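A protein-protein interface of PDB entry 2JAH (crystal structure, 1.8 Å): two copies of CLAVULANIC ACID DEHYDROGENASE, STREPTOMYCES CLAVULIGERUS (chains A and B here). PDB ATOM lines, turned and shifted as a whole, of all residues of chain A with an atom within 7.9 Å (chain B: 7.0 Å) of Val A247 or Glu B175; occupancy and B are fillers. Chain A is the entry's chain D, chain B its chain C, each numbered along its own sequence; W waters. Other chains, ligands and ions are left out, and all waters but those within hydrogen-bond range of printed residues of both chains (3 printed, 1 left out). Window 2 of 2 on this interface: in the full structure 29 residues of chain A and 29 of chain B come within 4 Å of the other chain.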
ATOM      1  N   ILE A 143     -12.346  -9.977   6.684  1.00  0.00           N
ATOM      2  CA  ILE A 143     -13.334 -10.266   5.622  1.00  0.00           C
ATOM      3  C   ILE A 143     -12.687 -11.080   4.484  1.00  0.00           C
ATOM      4  O   ILE A 143     -13.341 -11.913   3.830  1.00  0.00           O
ATOM      5  CB  ILE A 143     -14.000  -8.952   5.084  1.00  0.00           C
ATOM      6  CG1 ILE A 143     -15.153  -9.255   4.121  1.00  0.00           C
ATOM      7  CG2 ILE A 143     -12.952  -7.978   4.447  1.00  0.00           C
ATOM      8  CD1 ILE A 143     -16.094  -8.062   3.897  1.00  0.00           C
ATOM      9  N   VAL A 147     -14.545 -13.774   2.250  1.00  0.00           N
ATOM     10  CA  VAL A 147     -15.021 -13.272   0.948  1.00  0.00           C
ATOM     11  C   VAL A 147     -13.833 -12.990   0.024  1.00  0.00           C
ATOM     12  O   VAL A 147     -12.891 -12.318   0.425  1.00  0.00           O
ATOM     13  CB  VAL A 147     -15.814 -11.933   1.121  1.00  0.00           C
ATOM     14  CG1 VAL A 147     -16.387 -11.450  -0.216  1.00  0.00           C
ATOM     15  CG2 VAL A 147     -16.930 -12.093   2.165  1.00  0.00           C
ATOM     16  N   VAL A 149     -12.490 -11.030  -3.220  1.00  0.00           N
ATOM     17  CA  VAL A 149     -12.615  -9.997  -4.258  1.00  0.00           C
ATOM     18  C   VAL A 149     -11.364  -9.933  -5.139  1.00  0.00           C
ATOM     19  O   VAL A 149     -10.306 -10.445  -4.776  1.00  0.00           O
ATOM     20  CB  VAL A 149     -12.925  -8.587  -3.671  1.00  0.00           C
ATOM     21  CG1 VAL A 149     -14.203  -8.629  -2.837  1.00  0.00           C
ATOM     22  CG2 VAL A 149     -11.738  -8.046  -2.852  1.00  0.00           C
ATOM     23  N   ILE A 212     -17.440   5.415   2.354  1.00  0.00           N
ATOM     24  CA  ILE A 212     -18.037   4.761   3.516  1.00  0.00           C
ATOM     25  C   ILE A 212     -17.523   5.300   4.857  1.00  0.00           C
ATOM     26  O   ILE A 212     -16.410   5.834   4.944  1.00  0.00           O
ATOM     27  CB  ILE A 212     -17.836   3.222   3.458  1.00  0.00           C
ATOM     28  CG1 ILE A 212     -16.357   2.852   3.610  1.00  0.00           C
ATOM     29  CG2 ILE A 212     -18.404   2.665   2.145  1.00  0.00           C
ATOM     30  CD1 ILE A 212     -16.118   1.411   4.029  1.00  0.00           C
ATOM     31  N   ARG A 213     -18.344   5.176   5.897  1.00  0.00           N
ATOM     32  CA  ARG A 213     -17.838   5.287   7.256  1.00  0.00           C
ATOM     33  C   ARG A 213     -17.080   3.986   7.511  1.00  0.00           C
ATOM     34  O   ARG A 213     -17.676   2.895   7.523  1.00  0.00           O
ATOM     35  CB  ARG A 213     -18.978   5.455   8.263  1.00  0.00           C
ATOM     36  CG  ARG A 213     -19.836   6.706   8.062  1.00  0.00           C
ATOM     37  CD  ARG A 213     -21.135   6.619   8.878  1.00  0.00           C
ATOM     38  NE  ARG A 213     -22.002   5.521   8.434  1.00  0.00           N
ATOM     39  CZ  ARG A 213     -22.980   4.985   9.163  1.00  0.00           C
ATOM     40  NH1 ARG A 213     -23.227   5.433  10.385  1.00  0.00           N
ATOM     41  NH2 ARG A 213     -23.720   4.002   8.669  1.00  0.00           N
ATOM     42  N   ARG A 242     -18.499  -5.876   9.769  1.00  0.00           N
ATOM     43  CA  ARG A 242     -18.433  -5.210   8.462  1.00  0.00           C
ATOM     44  C   ARG A 242     -18.833  -3.745   8.631  1.00  0.00           C
ATOM     45  O   ARG A 242     -19.605  -3.415   9.530  1.00  0.00           O
ATOM     46  CB  ARG A 242     -19.434  -5.845   7.470  1.00  0.00           C
ATOM     47  CG  ARG A 242     -19.193  -7.272   7.032  1.00  0.00           C
ATOM     48  CD  ARG A 242     -20.309  -7.615   6.079  1.00  0.00           C
ATOM     49  NE  ARG A 242     -20.129  -8.841   5.314  1.00  0.00           N
ATOM     50  CZ  ARG A 242     -19.740  -8.891   4.044  1.00  0.00           C
ATOM     51  NH1 ARG A 242     -19.454  -7.784   3.378  1.00  0.00           N
ATOM     52  NH2 ARG A 242     -19.631 -10.064   3.441  1.00  0.00           N
ATOM     53  N   PRO A 243     -18.325  -2.858   7.758  1.00  0.00           N
ATOM     54  CA  PRO A 243     -18.883  -1.501   7.726  1.00  0.00           C
ATOM     55  C   PRO A 243     -20.336  -1.547   7.252  1.00  0.00           C
ATOM     56  O   PRO A 243     -20.636  -2.205   6.254  1.00  0.00           O
ATOM     57  CB  PRO A 243     -17.999  -0.767   6.702  1.00  0.00           C
ATOM     58  CG  PRO A 243     -16.814  -1.644   6.457  1.00  0.00           C
ATOM     59  CD  PRO A 243     -17.239  -3.054   6.782  1.00  0.00           C
ATOM     60  N   THR A 244     -21.242  -0.889   7.977  1.00  0.00           N
ATOM     61  CA  THR A 244     -22.665  -0.850   7.598  1.00  0.00           C
ATOM     62  C   THR A 244     -22.872  -0.259   6.200  1.00  0.00           C
ATOM     63  O   THR A 244     -23.782  -0.656   5.469  1.00  0.00           O
ATOM     64  CB  THR A 244     -23.504  -0.025   8.612  1.00  0.00           C
ATOM     65  OG1 THR A 244     -23.300  -0.532   9.936  1.00  0.00           O
ATOM     66  CG2 THR A 244     -24.997  -0.108   8.287  1.00  0.00           C
ATOM     67  N   ASP A 245     -22.022   0.694   5.840  1.00  0.00           N
ATOM     68  CA  ASP A 245     -22.158   1.403   4.578  1.00  0.00           C
ATOM     69  C   ASP A 245     -21.739   0.584   3.350  1.00  0.00           C
ATOM     70  O   ASP A 245     -21.967   1.002   2.217  1.00  0.00           O
ATOM     71  CB  ASP A 245     -21.343   2.703   4.630  1.00  0.00           C
ATOM     72  CG  ASP A 245     -21.915   3.720   5.601  1.00  0.00           C
ATOM     73  OD1 ASP A 245     -23.083   3.584   6.020  1.00  0.00           O
ATOM     74  OD2 ASP A 245     -21.186   4.677   5.941  1.00  0.00           O
ATOM     75  N   GLN A 246     -21.146  -0.581   3.571  1.00  0.00           N
ATOM     76  CA  GLN A 246     -20.468  -1.287   2.492  1.00  0.00           C
ATOM     77  C   GLN A 246     -21.160  -2.587   2.108  1.00  0.00           C
ATOM     78  O   GLN A 246     -21.181  -3.531   2.890  1.00  0.00           O
ATOM     79  CB  GLN A 246     -19.041  -1.578   2.928  1.00  0.00           C
ATOM     80  CG  GLN A 246     -18.160  -2.230   1.887  1.00  0.00           C
ATOM     81  CD  GLN A 246     -16.853  -2.667   2.499  1.00  0.00           C
ATOM     82  OE1 GLN A 246     -16.783  -3.703   3.175  1.00  0.00           O
ATOM     83  NE2 GLN A 246     -15.810  -1.878   2.289  1.00  0.00           N
ATOM     84  N   VAL A 247     -21.705  -2.631   0.893  1.00  0.00           N
ATOM     85  CA  VAL A 247     -22.252  -3.876   0.356  1.00  0.00           C
ATOM     86  C   VAL A 247     -21.108  -4.886   0.230  1.00  0.00           C
ATOM     87  O   VAL A 247     -21.186  -6.018   0.710  1.00  0.00           O
ATOM     88  CB  VAL A 247     -22.955  -3.677  -1.019  1.00  0.00           C
ATOM     89  CG1 VAL A 247     -23.416  -5.015  -1.605  1.00  0.00           C
ATOM     90  CG2 VAL A 247     -24.141  -2.768  -0.882  1.00  0.00           C
ATOM     91  OXT VAL A 247     -20.059  -4.578  -0.343  1.00  0.00           O
ATOM     92  N   LYS B 134     -33.416   3.208  10.971  1.00  0.00           N
ATOM     93  CA  LYS B 134     -32.055   2.704  10.729  1.00  0.00           C
ATOM     94  C   LYS B 134     -31.706   1.643  11.775  1.00  0.00           C
ATOM     95  O   LYS B 134     -30.676   1.693  12.472  1.00  0.00           O
ATOM     96  CB  LYS B 134     -31.035   3.847  10.650  1.00  0.00           C
ATOM     97  CG  LYS B 134     -31.122   4.618   9.334  1.00  0.00           C
ATOM     98  CD  LYS B 134     -30.041   5.679   9.229  1.00  0.00           C
ATOM     99  CE  LYS B 134     -30.092   6.389   7.875  1.00  0.00           C
ATOM    100  NZ  LYS B 134     -31.306   7.241   7.707  1.00  0.00           N
ATOM    101  N   GLU B 167     -27.594 -12.840   4.612  1.00  0.00           N
ATOM    102  CA  GLU B 167     -26.505 -12.172   3.869  1.00  0.00           C
ATOM    103  C   GLU B 167     -27.041 -11.406   2.668  1.00  0.00           C
ATOM    104  O   GLU B 167     -26.595 -10.274   2.383  1.00  0.00           O
ATOM    105  CB  GLU B 167     -25.397 -13.150   3.461  1.00  0.00           C
ATOM    106  CG  GLU B 167     -24.456 -12.656   2.333  1.00  0.00           C
ATOM    107  CD  GLU B 167     -23.738 -11.332   2.636  1.00  0.00           C
ATOM    108  OE1 GLU B 167     -23.646 -10.905   3.812  1.00  0.00           O
ATOM    109  OE2 GLU B 167     -23.249 -10.714   1.678  1.00  0.00           O
ATOM    110  N   ARG B 170     -28.713  -8.289   3.939  1.00  0.00           N
ATOM    111  CA  ARG B 170     -27.670  -7.293   4.244  1.00  0.00           C
ATOM    112  C   ARG B 170     -27.260  -6.539   2.985  1.00  0.00           C
ATOM    113  O   ARG B 170     -27.239  -5.299   2.963  1.00  0.00           O
ATOM    114  CB  ARG B 170     -26.445  -7.951   4.886  1.00  0.00           C
ATOM    115  CG  ARG B 170     -25.372  -6.950   5.350  1.00  0.00           C
ATOM    116  CD  ARG B 170     -24.034  -7.651   5.594  1.00  0.00           C
ATOM    117  NE  ARG B 170     -23.516  -8.172   4.340  1.00  0.00           N
ATOM    118  CZ  ARG B 170     -22.881  -7.437   3.427  1.00  0.00           C
ATOM    119  NH1 ARG B 170     -22.621  -6.147   3.645  1.00  0.00           N
ATOM    120  NH2 ARG B 170     -22.483  -8.002   2.299  1.00  0.00           N
ATOM    121  N   GLN B 171     -26.961  -7.269   1.919  1.00  0.00           N
ATOM    122  CA  GLN B 171     -26.618  -6.611   0.652  1.00  0.00           C
ATOM    123  C   GLN B 171     -27.695  -5.622   0.169  1.00  0.00           C
ATOM    124  O   GLN B 171     -27.373  -4.552  -0.347  1.00  0.00           O
ATOM    125  CB  GLN B 171     -26.318  -7.635  -0.444  1.00  0.00           C
ATOM    126  CG  GLN B 171     -25.082  -8.483  -0.212  1.00  0.00           C
ATOM    127  CD  GLN B 171     -24.859  -9.485  -1.328  1.00  0.00           C
ATOM    128  OE1 GLN B 171     -25.224  -9.239  -2.477  1.00  0.00           O
ATOM    129  NE2 GLN B 171     -24.255 -10.619  -0.998  1.00  0.00           N
ATOM    130  N   GLU B 172     -28.961  -5.982   0.369  1.00  0.00           N
ATOM    131  CA  GLU B 172     -30.110  -5.189  -0.076  1.00  0.00           C
ATOM    132  C   GLU B 172     -30.436  -3.952   0.778  1.00  0.00           C
ATOM    133  O   GLU B 172     -30.929  -2.938   0.263  1.00  0.00           O
ATOM    134  CB  GLU B 172     -31.348  -6.078  -0.129  1.00  0.00           C
ATOM    135  CG  GLU B 172     -31.407  -6.995  -1.353  1.00  0.00           C
ATOM    136  CD  GLU B 172     -32.585  -7.954  -1.310  1.00  0.00           C
ATOM    137  OE1 GLU B 172     -33.627  -7.616  -0.682  1.00  0.00           O
ATOM    138  OE2 GLU B 172     -32.469  -9.049  -1.911  1.00  0.00           O
ATOM    139  N   VAL B 173     -30.183  -4.031   2.078  1.00  0.00           N
ATOM    140  CA  VAL B 173     -30.631  -2.954   2.982  1.00  0.00           C
ATOM    141  C   VAL B 173     -29.511  -2.196   3.698  1.00  0.00           C
ATOM    142  O   VAL B 173     -29.771  -1.143   4.315  1.00  0.00           O
ATOM    143  CB  VAL B 173     -31.684  -3.464   4.045  1.00  0.00           C
ATOM    144  CG1 VAL B 173     -32.913  -4.068   3.369  1.00  0.00           C
ATOM    145  CG2 VAL B 173     -31.069  -4.466   5.033  1.00  0.00           C
ATOM    146  N   THR B 174     -28.282  -2.717   3.652  1.00  0.00           N
ATOM    147  CA  THR B 174     -27.230  -2.162   4.521  1.00  0.00           C
ATOM    148  C   THR B 174     -26.913  -0.704   4.188  1.00  0.00           C
ATOM    149  O   THR B 174     -26.655   0.093   5.088  1.00  0.00           O
ATOM    150  CB  THR B 174     -25.940  -3.039   4.627  1.00  0.00           C
ATOM    151  OG1 THR B 174     -25.206  -2.660   5.806  1.00  0.00           O
ATOM    152  CG2 THR B 174     -25.039  -2.913   3.363  1.00  0.00           C
ATOM    153  N   GLU B 175     -26.985  -0.343   2.908  1.00  0.00           N
ATOM    154  CA  GLU B 175     -26.695   1.038   2.514  1.00  0.00           C
ATOM    155  C   GLU B 175     -27.757   2.016   3.027  1.00  0.00           C
ATOM    156  O   GLU B 175     -27.494   3.207   3.139  1.00  0.00           O
ATOM    157  CB  GLU B 175     -26.542   1.156   0.999  1.00  0.00           C
ATOM    158  CG  GLU B 175     -25.319   0.453   0.443  1.00  0.00           C
ATOM    159  CD  GLU B 175     -25.444   0.200  -1.045  1.00  0.00           C
ATOM    160  OE1 GLU B 175     -26.438  -0.439  -1.455  1.00  0.00           O
ATOM    161  OE2 GLU B 175     -24.553   0.638  -1.809  1.00  0.00           O
ATOM    162  N   ARG B 176     -28.950   1.510   3.340  1.00  0.00           N
ATOM    163  CA  ARG B 176     -30.014   2.356   3.899  1.00  0.00           C
ATOM    164  C   ARG B 176     -30.000   2.324   5.435  1.00  0.00           C
ATOM    165  O   ARG B 176     -30.911   2.828   6.097  1.00  0.00           O
ATOM    166  CB  ARG B 176     -31.381   1.972   3.314  1.00  0.00           C
ATOM    167  CG  ARG B 176     -31.586   2.489   1.897  1.00  0.00           C
ATOM    168  CD  ARG B 176     -32.852   1.952   1.289  1.00  0.00           C
ATOM    169  NE  ARG B 176     -32.727   0.515   1.032  1.00  0.00           N
ATOM    170  CZ  ARG B 176     -33.750  -0.306   0.826  1.00  0.00           C
ATOM    171  NH1 ARG B 176     -34.999   0.143   0.861  1.00  0.00           N
ATOM    172  NH2 ARG B 176     -33.517  -1.587   0.596  1.00  0.00           N
ATOM    173  N   GLY B 177     -28.947   1.734   5.994  1.00  0.00           N
ATOM    174  CA  GLY B 177     -28.702   1.808   7.427  1.00  0.00           C
ATOM    175  C   GLY B 177     -29.362   0.752   8.298  1.00  0.00           C
ATOM    176  O   GLY B 177     -29.311   0.859   9.529  1.00  0.00           O
ATOM    177  N   VAL B 178     -29.971  -0.261   7.680  1.00  0.00           N
ATOM    178  CA  VAL B 178     -30.510  -1.399   8.430  1.00  0.00           C
ATOM    179  C   VAL B 178     -29.400  -2.442   8.601  1.00  0.00           C
ATOM    180  O   VAL B 178     -28.878  -2.982   7.627  1.00  0.00           O
ATOM    181  CB  VAL B 178     -31.752  -2.047   7.748  1.00  0.00           C
ATOM    182  CG1 VAL B 178     -32.212  -3.296   8.540  1.00  0.00           C
ATOM    183  CG2 VAL B 178     -32.895  -1.048   7.626  1.00  0.00           C
HETATM  184  O   HOH W   1     -22.629  -4.339   5.967  1.00  0.00           O
HETATM  185  O   HOH W   2     -25.411   2.453   6.088  1.00  0.00           O
HETATM  186  O   HOH W   3     -20.639 -11.147   1.291  1.00  0.00           O
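O of Thr A244 lies within hydrogen-bond range of OG1 of Thr B174 (2.5 Å).
The guanidinium group of Arg B170 sits at hydrogen-bond distance from the backbone carbonyl oxygen of Gln A246 (3.1 Å).
The chain-end carboxylate (O) of Val A247 lies within salt-bridge range of the guanidinium group (NH2) of Arg B170, 2.9 Å away.
The guanidinium group of Arg B170 sits close to the guanidinium group of Arg A242, 3.2 Å away.
The chain-end carboxylate of Val A247 is in salt-bridge range of the guanidinium group of Arg A242, at 3.6 Å.
The side-chain carboxylate of Glu B167 sits at hydrogen-bond distance from the side-chain amide nitrogen of Gln B171 (2.9 Å).
The side-chain carboxylate of Glu B167 is in salt-bridge range of the guanidinium group of Arg B170.
The guanidinium group (NH2) of Arg A213 is in salt-bridge range of the side-chain carboxylate (OD1) of Asp A245 (2.8 Å).
O of Asp A245 touches CG of Glu B175 (3.8 Å).
Gln A246 touches Thr B174 (O to CG2, 3.9 Å).
CG2 of Val A247 touches O of Gln B171, 3.7 Å away.
Glu B175 touches Val A247.
Printed residues of chain B within 4 Å of Val A247: Arg B170, Gln B171 and Glu B175.
Of chain A, only Asp A245 (3.8 Å) and Val A247 (3.2 Å) come within 4 Å of Glu B175.
Printed residues of chain A within 4 Å of Gln B171: Val A247 (3.7 Å).
Printed residues of chain A within 4 Å of Arg B170: Arg A242 (3.2 Å), Gln A246 (3.1 Å) and Val A247 (2.9 Å).
Of the printed residues of chain B, Asp A245 touches Glu B175.
Printed residues of chain B within 4 Å of Thr A244: Thr B174 (2.5 Å).
The nearest residue of chain B that does not touch Val A247 is Thr B174 (4.2 Å).
The nearest residue of chain A that does not touch Glu B175 is Thr A244 (4.1 Å).
Of the 11 printed residues of chain B, 4 touch a printed residue of chain A.
Among the printed residues, no Asp or Glu carboxylate lies within 4 Å of a Lys or Arg side-chain nitrogen of the other chain.
No position is printed for both chains.
Of the 8 pairs that touch across the chains among the printed residues, none has its exchanged pair printed and touching as well.
Water W2 lies within hydrogen-bond range of OD1 of Asp A245, O of Thr B174 and NH2 of Arg A213.
Water W3 bridges NH2 of Arg A242 (2.6 Å) and OE2 of Glu B167 (2.7 Å).
Water W1 lies within hydrogen-bond range of O of Pro A243, NH1 of Arg B170, OG1 of Thr B174 and O of Gln A246.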
